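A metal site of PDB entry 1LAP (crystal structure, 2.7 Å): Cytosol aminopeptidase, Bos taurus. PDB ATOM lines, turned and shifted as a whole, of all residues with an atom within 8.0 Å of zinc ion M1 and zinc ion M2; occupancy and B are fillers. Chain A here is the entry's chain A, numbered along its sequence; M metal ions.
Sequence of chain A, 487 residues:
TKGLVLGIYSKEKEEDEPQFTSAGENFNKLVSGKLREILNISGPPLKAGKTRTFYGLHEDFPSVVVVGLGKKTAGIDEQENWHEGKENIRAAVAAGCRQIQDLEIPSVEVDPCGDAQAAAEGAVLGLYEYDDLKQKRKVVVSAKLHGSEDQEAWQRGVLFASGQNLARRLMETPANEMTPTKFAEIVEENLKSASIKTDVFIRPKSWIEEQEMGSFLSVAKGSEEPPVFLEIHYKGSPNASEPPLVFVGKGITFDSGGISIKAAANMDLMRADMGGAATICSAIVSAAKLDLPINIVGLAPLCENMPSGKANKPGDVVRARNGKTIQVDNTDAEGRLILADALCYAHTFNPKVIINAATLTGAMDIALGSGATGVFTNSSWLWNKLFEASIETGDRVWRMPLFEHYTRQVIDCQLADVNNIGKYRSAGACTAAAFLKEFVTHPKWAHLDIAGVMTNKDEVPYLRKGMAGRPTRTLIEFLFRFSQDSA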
ATOM      1  N   VAL A 219      30.478  -5.413   8.166  1.00  0.00           N
ATOM      2  CA  VAL A 219      30.297  -6.851   8.173  1.00  0.00           C
ATOM      3  C   VAL A 219      31.471  -7.457   7.446  1.00  0.00           C
ATOM      4  O   VAL A 219      32.162  -8.313   8.010  1.00  0.00           O
ATOM      5  CB  VAL A 219      29.007  -7.262   7.459  1.00  0.00           C
ATOM      6  CG1 VAL A 219      28.886  -8.778   7.373  1.00  0.00           C
ATOM      7  CG2 VAL A 219      27.833  -6.799   8.300  1.00  0.00           C
ATOM      8  N   LYS A 250      19.967 -10.105   0.196  1.00  0.00           N
ATOM      9  CA  LYS A 250      21.064 -10.288   1.129  1.00  0.00           C
ATOM     10  C   LYS A 250      21.988 -11.337   0.495  1.00  0.00           C
ATOM     11  O   LYS A 250      21.500 -12.431   0.159  1.00  0.00           O
ATOM     12  CB  LYS A 250      20.464 -10.780   2.459  1.00  0.00           C
ATOM     13  CG  LYS A 250      21.445 -11.230   3.571  1.00  0.00           C
ATOM     14  CD  LYS A 250      20.698 -11.781   4.752  1.00  0.00           C
ATOM     15  CE  LYS A 250      21.807 -12.257   5.614  1.00  0.00           C
ATOM     16  NZ  LYS A 250      21.334 -13.127   6.670  1.00  0.00           N
ATOM     17  N   GLY A 251      23.262 -11.046   0.256  1.00  0.00           N
ATOM     18  CA  GLY A 251      24.170 -12.032  -0.245  1.00  0.00           C
ATOM     19  C   GLY A 251      25.258 -12.314   0.757  1.00  0.00           C
ATOM     20  O   GLY A 251      26.422 -11.917   0.554  1.00  0.00           O
ATOM     21  N   ILE A 252      24.946 -12.981   1.882  1.00  0.00           N
ATOM     22  CA  ILE A 252      26.043 -13.331   2.774  1.00  0.00           C
ATOM     23  C   ILE A 252      26.442 -14.681   2.223  1.00  0.00           C
ATOM     24  O   ILE A 252      25.577 -15.521   2.047  1.00  0.00           O
ATOM     25  CB  ILE A 252      25.581 -13.377   4.261  1.00  0.00           C
ATOM     26  CG1 ILE A 252      25.205 -11.944   4.609  1.00  0.00           C
ATOM     27  CG2 ILE A 252      26.689 -13.805   5.261  1.00  0.00           C
ATOM     28  CD1 ILE A 252      26.404 -10.967   4.749  1.00  0.00           C
ATOM     29  N   THR A 253      27.703 -14.933   1.849  1.00  0.00           N
ATOM     30  CA  THR A 253      28.018 -16.160   1.173  1.00  0.00           C
ATOM     31  C   THR A 253      28.355 -17.285   2.095  1.00  0.00           C
ATOM     32  O   THR A 253      28.331 -18.462   1.745  1.00  0.00           O
ATOM     33  CB  THR A 253      29.138 -15.843   0.150  1.00  0.00           C
ATOM     34  OG1 THR A 253      30.187 -15.107   0.757  1.00  0.00           O
ATOM     35  CG2 THR A 253      28.501 -15.039  -1.044  1.00  0.00           C
ATOM     36  N   PHE A 254      28.672 -16.885   3.307  1.00  0.00           N
ATOM     37  CA  PHE A 254      28.740 -17.814   4.406  1.00  0.00           C
ATOM     38  C   PHE A 254      28.571 -16.968   5.640  1.00  0.00           C
ATOM     39  O   PHE A 254      29.244 -15.924   5.813  1.00  0.00           O
ATOM     40  CB  PHE A 254      30.109 -18.546   4.555  1.00  0.00           C
ATOM     41  CG  PHE A 254      30.004 -19.577   5.701  1.00  0.00           C
ATOM     42  CD1 PHE A 254      29.142 -20.650   5.558  1.00  0.00           C
ATOM     43  CD2 PHE A 254      30.683 -19.366   6.886  1.00  0.00           C
ATOM     44  CE1 PHE A 254      28.886 -21.466   6.619  1.00  0.00           C
ATOM     45  CE2 PHE A 254      30.470 -20.204   7.947  1.00  0.00           C
ATOM     46  CZ  PHE A 254      29.557 -21.235   7.811  1.00  0.00           C
ATOM     47  N   ASP A 255      27.706 -17.466   6.516  1.00  0.00           N
ATOM     48  CA  ASP A 255      27.574 -16.790   7.801  1.00  0.00           C
ATOM     49  C   ASP A 255      28.000 -17.660   8.973  1.00  0.00           C
ATOM     50  O   ASP A 255      27.344 -18.665   9.332  1.00  0.00           O
ATOM     51  CB  ASP A 255      26.156 -16.360   7.986  1.00  0.00           C
ATOM     52  CG  ASP A 255      25.859 -15.494   9.187  1.00  0.00           C
ATOM     53  OD1 ASP A 255      24.670 -15.455   9.432  1.00  0.00           O
ATOM     54  OD2 ASP A 255      26.730 -14.897   9.824  1.00  0.00           O
ATOM     55  N   SER A 256      29.112 -17.244   9.567  1.00  0.00           N
ATOM     56  CA  SER A 256      29.576 -17.981  10.727  1.00  0.00           C
ATOM     57  C   SER A 256      28.945 -17.420  11.975  1.00  0.00           C
ATOM     58  O   SER A 256      28.987 -18.073  13.012  1.00  0.00           O
ATOM     59  CB  SER A 256      31.088 -17.895  10.873  1.00  0.00           C
ATOM     60  OG  SER A 256      31.449 -16.528  11.060  1.00  0.00           O
ATOM     61  N   GLY A 257      28.433 -16.179  11.897  1.00  0.00           N
ATOM     62  CA  GLY A 257      27.971 -15.427  13.075  1.00  0.00           C
ATOM     63  C   GLY A 257      28.916 -14.261  13.472  1.00  0.00           C
ATOM     64  O   GLY A 257      28.543 -13.204  14.038  1.00  0.00           O
ATOM     65  N   GLY A 258      30.179 -14.403  13.064  1.00  0.00           N
ATOM     66  CA  GLY A 258      31.182 -13.460  13.430  1.00  0.00           C
ATOM     67  C   GLY A 258      31.597 -13.845  14.834  1.00  0.00           C
ATOM     68  O   GLY A 258      31.748 -15.041  15.123  1.00  0.00           O
ATOM     69  N   SER A 260      29.797 -13.007  17.512  1.00  0.00           N
ATOM     70  CA  SER A 260      28.627 -13.696  18.072  1.00  0.00           C
ATOM     71  C   SER A 260      28.486 -15.043  17.299  1.00  0.00           C
ATOM     72  O   SER A 260      27.468 -15.332  16.636  1.00  0.00           O
ATOM     73  CB  SER A 260      27.442 -12.829  17.864  1.00  0.00           C
ATOM     74  OG  SER A 260      27.677 -11.444  18.156  1.00  0.00           O
ATOM     75  N   LYS A 262      28.031 -18.651  15.649  1.00  0.00           N
ATOM     76  CA  LYS A 262      26.988 -19.621  15.526  1.00  0.00           C
ATOM     77  C   LYS A 262      27.337 -20.921  16.263  1.00  0.00           C
ATOM     78  O   LYS A 262      28.506 -21.229  16.531  1.00  0.00           O
ATOM     79  CB  LYS A 262      26.791 -19.901  14.065  1.00  0.00           C
ATOM     80  CG  LYS A 262      25.461 -19.500  13.452  1.00  0.00           C
ATOM     81  CD  LYS A 262      25.707 -18.448  12.421  1.00  0.00           C
ATOM     82  CE  LYS A 262      24.507 -18.163  11.548  1.00  0.00           C
ATOM     83  NZ  LYS A 262      23.356 -17.745  12.331  1.00  0.00           N
ATOM     84  N   MET A 270      24.617 -22.329   6.300  1.00  0.00           N
ATOM     85  CA  MET A 270      24.711 -20.894   6.102  1.00  0.00           C
ATOM     86  C   MET A 270      25.461 -20.592   4.805  1.00  0.00           C
ATOM     87  O   MET A 270      25.679 -19.437   4.438  1.00  0.00           O
ATOM     88  CB  MET A 270      25.400 -20.250   7.301  1.00  0.00           C
ATOM     89  CG  MET A 270      24.618 -20.280   8.611  1.00  0.00           C
ATOM     90  SD  MET A 270      22.834 -19.953   8.492  1.00  0.00           S
ATOM     91  CE  MET A 270      22.770 -18.220   8.678  1.00  0.00           C
ATOM     92  N   ALA A 272      23.894 -21.081   2.412  1.00  0.00           N
ATOM     93  CA  ALA A 272      22.721 -20.563   1.799  1.00  0.00           C
ATOM     94  C   ALA A 272      22.238 -19.241   2.316  1.00  0.00           C
ATOM     95  O   ALA A 272      21.123 -18.857   1.944  1.00  0.00           O
ATOM     96  CB  ALA A 272      21.624 -21.545   1.947  1.00  0.00           C
ATOM     97  N   ASP A 273      23.067 -18.454   3.029  1.00  0.00           N
ATOM     98  CA  ASP A 273      22.662 -17.157   3.533  1.00  0.00           C
ATOM     99  C   ASP A 273      22.724 -16.112   2.399  1.00  0.00           C
ATOM    100  O   ASP A 273      22.660 -14.897   2.572  1.00  0.00           O
ATOM    101  CB  ASP A 273      23.589 -16.788   4.718  1.00  0.00           C
ATOM    102  CG  ASP A 273      22.868 -15.964   5.782  1.00  0.00           C
ATOM    103  OD1 ASP A 273      23.473 -15.084   6.405  1.00  0.00           O
ATOM    104  OD2 ASP A 273      21.677 -16.203   5.986  1.00  0.00           O
ATOM    105  N   MET A 274      22.995 -16.524   1.183  1.00  0.00           N
ATOM    106  CA  MET A 274      22.948 -15.598   0.073  1.00  0.00           C
ATOM    107  C   MET A 274      21.719 -15.952  -0.751  1.00  0.00           C
ATOM    108  O   MET A 274      21.540 -15.412  -1.845  1.00  0.00           O
ATOM    109  CB  MET A 274      24.247 -15.663  -0.802  1.00  0.00           C
ATOM    110  CG  MET A 274      24.899 -17.057  -0.916  1.00  0.00           C
ATOM    111  SD  MET A 274      23.825 -18.387  -1.537  1.00  0.00           S
ATOM    112  CE  MET A 274      23.843 -17.725  -3.169  1.00  0.00           C
ATOM    113  N   ASN A 305      30.513 -13.475   6.546  1.00  0.00           N
ATOM    114  CA  ASN A 305      30.584 -12.939   7.899  1.00  0.00           C
ATOM    115  C   ASN A 305      31.422 -13.863   8.773  1.00  0.00           C
ATOM    116  O   ASN A 305      30.944 -14.906   9.176  1.00  0.00           O
ATOM    117  CB  ASN A 305      29.173 -12.775   8.441  1.00  0.00           C
ATOM    118  CG  ASN A 305      29.105 -12.269   9.881  1.00  0.00           C
ATOM    119  OD1 ASN A 305      28.249 -12.659  10.659  1.00  0.00           O
ATOM    120  ND2 ASN A 305      29.977 -11.384  10.323  1.00  0.00           N
ATOM    121  N   ASN A 330      24.784  -7.577  18.255  1.00  0.00           N
ATOM    122  CA  ASN A 330      25.031  -8.967  17.977  1.00  0.00           C
ATOM    123  C   ASN A 330      25.510  -8.977  16.518  1.00  0.00           C
ATOM    124  O   ASN A 330      24.845  -8.462  15.590  1.00  0.00           O
ATOM    125  CB  ASN A 330      23.727  -9.729  18.185  1.00  0.00           C
ATOM    126  CG  ASN A 330      23.665 -11.069  17.476  1.00  0.00           C
ATOM    127  OD1 ASN A 330      24.629 -11.805  17.420  1.00  0.00           O
ATOM    128  ND2 ASN A 330      22.572 -11.447  16.830  1.00  0.00           N
ATOM    129  N   THR A 331      26.667  -9.590  16.300  1.00  0.00           N
ATOM    130  CA  THR A 331      27.281  -9.600  14.968  1.00  0.00           C
ATOM    131  C   THR A 331      26.607 -10.580  13.999  1.00  0.00           C
ATOM    132  O   THR A 331      26.793 -10.494  12.785  1.00  0.00           O
ATOM    133  CB  THR A 331      28.829  -9.883  15.100  1.00  0.00           C
ATOM    134  OG1 THR A 331      29.042 -11.160  15.677  1.00  0.00           O
ATOM    135  CG2 THR A 331      29.498  -8.956  16.092  1.00  0.00           C
ATOM    136  N   ASP A 332      25.786 -11.507  14.567  1.00  0.00           N
ATOM    137  CA  ASP A 332      25.042 -12.458  13.743  1.00  0.00           C
ATOM    138  C   ASP A 332      23.799 -11.768  13.159  1.00  0.00           C
ATOM    139  O   ASP A 332      23.108 -12.308  12.331  1.00  0.00           O
ATOM    140  CB  ASP A 332      24.675 -13.695  14.595  1.00  0.00           C
ATOM    141  CG  ASP A 332      24.283 -14.958  13.831  1.00  0.00           C
ATOM    142  OD1 ASP A 332      23.702 -15.843  14.455  1.00  0.00           O
ATOM    143  OD2 ASP A 332      24.563 -15.073  12.645  1.00  0.00           O
ATOM    144  N   ALA A 333      23.473 -10.521  13.530  1.00  0.00           N
ATOM    145  CA  ALA A 333      22.357  -9.817  12.900  1.00  0.00           C
ATOM    146  C   ALA A 333      22.998  -8.907  11.831  1.00  0.00           C
ATOM    147  O   ALA A 333      22.784  -7.702  11.698  1.00  0.00           O
ATOM    148  CB  ALA A 333      21.602  -9.015  13.959  1.00  0.00           C
ATOM    149  N   GLU A 334      23.813  -9.581  10.991  1.00  0.00           N
ATOM    150  CA  GLU A 334      24.534  -8.880   9.944  1.00  0.00           C
ATOM    151  C   GLU A 334      23.767  -8.535   8.663  1.00  0.00           C
ATOM    152  O   GLU A 334      23.953  -7.483   8.077  1.00  0.00           O
ATOM    153  CB  GLU A 334      25.831  -9.679   9.596  1.00  0.00           C
ATOM    154  CG  GLU A 334      25.841 -10.777   8.501  1.00  0.00           C
ATOM    155  CD  GLU A 334      24.951 -11.947   8.855  1.00  0.00           C
ATOM    156  OE1 GLU A 334      24.266 -12.459   7.986  1.00  0.00           O
ATOM    157  OE2 GLU A 334      24.967 -12.291  10.025  1.00  0.00           O
ATOM    158  N   GLY A 335      22.936  -9.393   8.100  1.00  0.00           N
ATOM    159  CA  GLY A 335      22.136  -9.070   6.934  1.00  0.00           C
ATOM    160  C   GLY A 335      21.361  -7.787   6.974  1.00  0.00           C
ATOM    161  O   GLY A 335      21.277  -7.128   5.943  1.00  0.00           O
ATOM    162  N   ARG A 336      20.826  -7.499   8.162  1.00  0.00           N
ATOM    163  CA  ARG A 336      20.162  -6.266   8.587  1.00  0.00           C
ATOM    164  C   ARG A 336      21.095  -5.118   8.146  1.00  0.00           C
ATOM    165  O   ARG A 336      20.782  -4.196   7.373  1.00  0.00           O
ATOM    166  CB  ARG A 336      20.010  -6.267  10.165  1.00  0.00           C
ATOM    167  CG  ARG A 336      18.732  -6.740  10.899  1.00  0.00           C
ATOM    168  CD  ARG A 336      18.760  -7.696  12.137  1.00  0.00           C
ATOM    169  NE  ARG A 336      18.528  -9.139  11.890  1.00  0.00           N
ATOM    170  CZ  ARG A 336      19.255  -9.918  11.005  1.00  0.00           C
ATOM    171  NH1 ARG A 336      18.959 -11.184  10.748  1.00  0.00           N
ATOM    172  NH2 ARG A 336      20.338  -9.519  10.329  1.00  0.00           N
ATOM    173  N   ILE A 338      23.706  -5.087   6.240  1.00  0.00           N
ATOM    174  CA  ILE A 338      24.070  -5.062   4.812  1.00  0.00           C
ATOM    175  C   ILE A 338      23.004  -4.424   3.915  1.00  0.00           C
ATOM    176  O   ILE A 338      23.237  -3.524   3.080  1.00  0.00           O
ATOM    177  CB  ILE A 338      24.442  -6.541   4.561  1.00  0.00           C
ATOM    178  CG1 ILE A 338      25.905  -6.340   4.459  1.00  0.00           C
ATOM    179  CG2 ILE A 338      23.880  -7.348   3.389  1.00  0.00           C
ATOM    180  CD1 ILE A 338      26.625  -7.579   4.974  1.00  0.00           C
ATOM    181  N   ALA A 358      15.694 -11.900   1.871  1.00  0.00           N
ATOM    182  CA  ALA A 358      16.741 -12.264   2.797  1.00  0.00           C
ATOM    183  C   ALA A 358      16.387 -13.460   3.661  1.00  0.00           C
ATOM    184  O   ALA A 358      15.271 -13.618   4.119  1.00  0.00           O
ATOM    185  CB  ALA A 358      17.026 -11.120   3.723  1.00  0.00           C
ATOM    186  N   THR A 359      17.359 -14.319   3.934  1.00  0.00           N
ATOM    187  CA  THR A 359      17.264 -15.459   4.802  1.00  0.00           C
ATOM    188  C   THR A 359      17.617 -14.718   6.090  1.00  0.00           C
ATOM    189  O   THR A 359      18.721 -14.817   6.613  1.00  0.00           O
ATOM    190  CB  THR A 359      18.338 -16.507   4.380  1.00  0.00           C
ATOM    191  OG1 THR A 359      19.413 -15.729   3.897  1.00  0.00           O
ATOM    192  CG2 THR A 359      17.898 -17.514   3.323  1.00  0.00           C
ATOM    193  N   LEU A 360      16.695 -13.917   6.608  1.00  0.00           N
ATOM    194  CA  LEU A 360      17.070 -13.060   7.699  1.00  0.00           C
ATOM    195  C   LEU A 360      17.070 -13.682   9.054  1.00  0.00           C
ATOM    196  O   LEU A 360      18.018 -13.556   9.804  1.00  0.00           O
ATOM    197  CB  LEU A 360      16.157 -11.856   7.809  1.00  0.00           C
ATOM    198  CG  LEU A 360      16.671 -10.465   7.539  1.00  0.00           C
ATOM    199  CD1 LEU A 360      15.983  -9.586   8.564  1.00  0.00           C
ATOM    200  CD2 LEU A 360      18.195 -10.360   7.575  1.00  0.00           C
ATOM    201  N   THR A 361      16.044 -14.478   9.341  1.00  0.00           N
ATOM    202  CA  THR A 361      15.766 -14.724  10.704  1.00  0.00           C
ATOM    203  C   THR A 361      15.309 -16.121  10.916  1.00  0.00           C
ATOM    204  O   THR A 361      14.387 -16.516  10.251  1.00  0.00           O
ATOM    205  CB  THR A 361      14.764 -13.554  10.941  1.00  0.00           C
ATOM    206  OG1 THR A 361      15.350 -12.847  11.979  1.00  0.00           O
ATOM    207  CG2 THR A 361      13.350 -13.892  11.273  1.00  0.00           C
HETATM  208 ZN    ZN M   1      23.998 -13.891  10.719  1.00  0.00          ZN
HETATM  209 ZN    ZN M   2      22.955 -13.935   8.024  1.00  0.00          ZN
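Zinc ion M1 is bound by OE2 of Glu 334 (2.0 Å). OD1 of Asp 255 is bound to zinc ion M1, 2.1 Å away. OD2 of Asp 332 is bound to zinc ion M1, 2.3 Å away. O of Asp 332 binds zinc ion M1 (2.4 Å).
OE1 of Glu 334 binds zinc ion M2 (2.0 Å). OD1 of Asp 273 is bound to zinc ion M2 (2.1 Å). NZ of Lys 250 is bound to zinc ion M2, at 2.3 Å. Slightly farther from zinc ion M2 lies OD1 of Asp 255 (2.7 Å).
OE2 of Glu 334 sits close to OD1 of Asn 305 (3.4 Å). The backbone carbonyl oxygen (O) of Asp 273 lies within hydrogen-bond range of the backbone NH (N) of Ile 252, at 3.1 Å. The side-chain carboxylate (OD1) of Asp 255 lies close to the side-chain amino group (NZ) of Lys 262, at 3.9 Å. The side-chain amide oxygen (OD1) of Asn 305 sits close to the side-chain carboxylate (OD2) of Asp 255 (2.8 Å). OD2 of Asp 255 sits at hydrogen-bond distance from N of Gly 257. The backbone carbonyl oxygen (O) of Thr 359 lies close to the side-chain amino group (NZ) of Lys 250 (3.1 Å). OD1 of Asp 332 lies within salt-bridge range of NZ of Lys 262, 2.9 Å away. N of Asp 332 sits at hydrogen-bond distance from O of Gly 257 (3.3 Å).
The nearest printed residue that does not touch zinc ion M2 is Met 270 (4.3 Å).
Within 4 Å of zinc ion M1: Asp 255, Asp 332 and Glu 334. Along chain A the residues within 4 Å of zinc ion M1 span positions 255 to 334.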
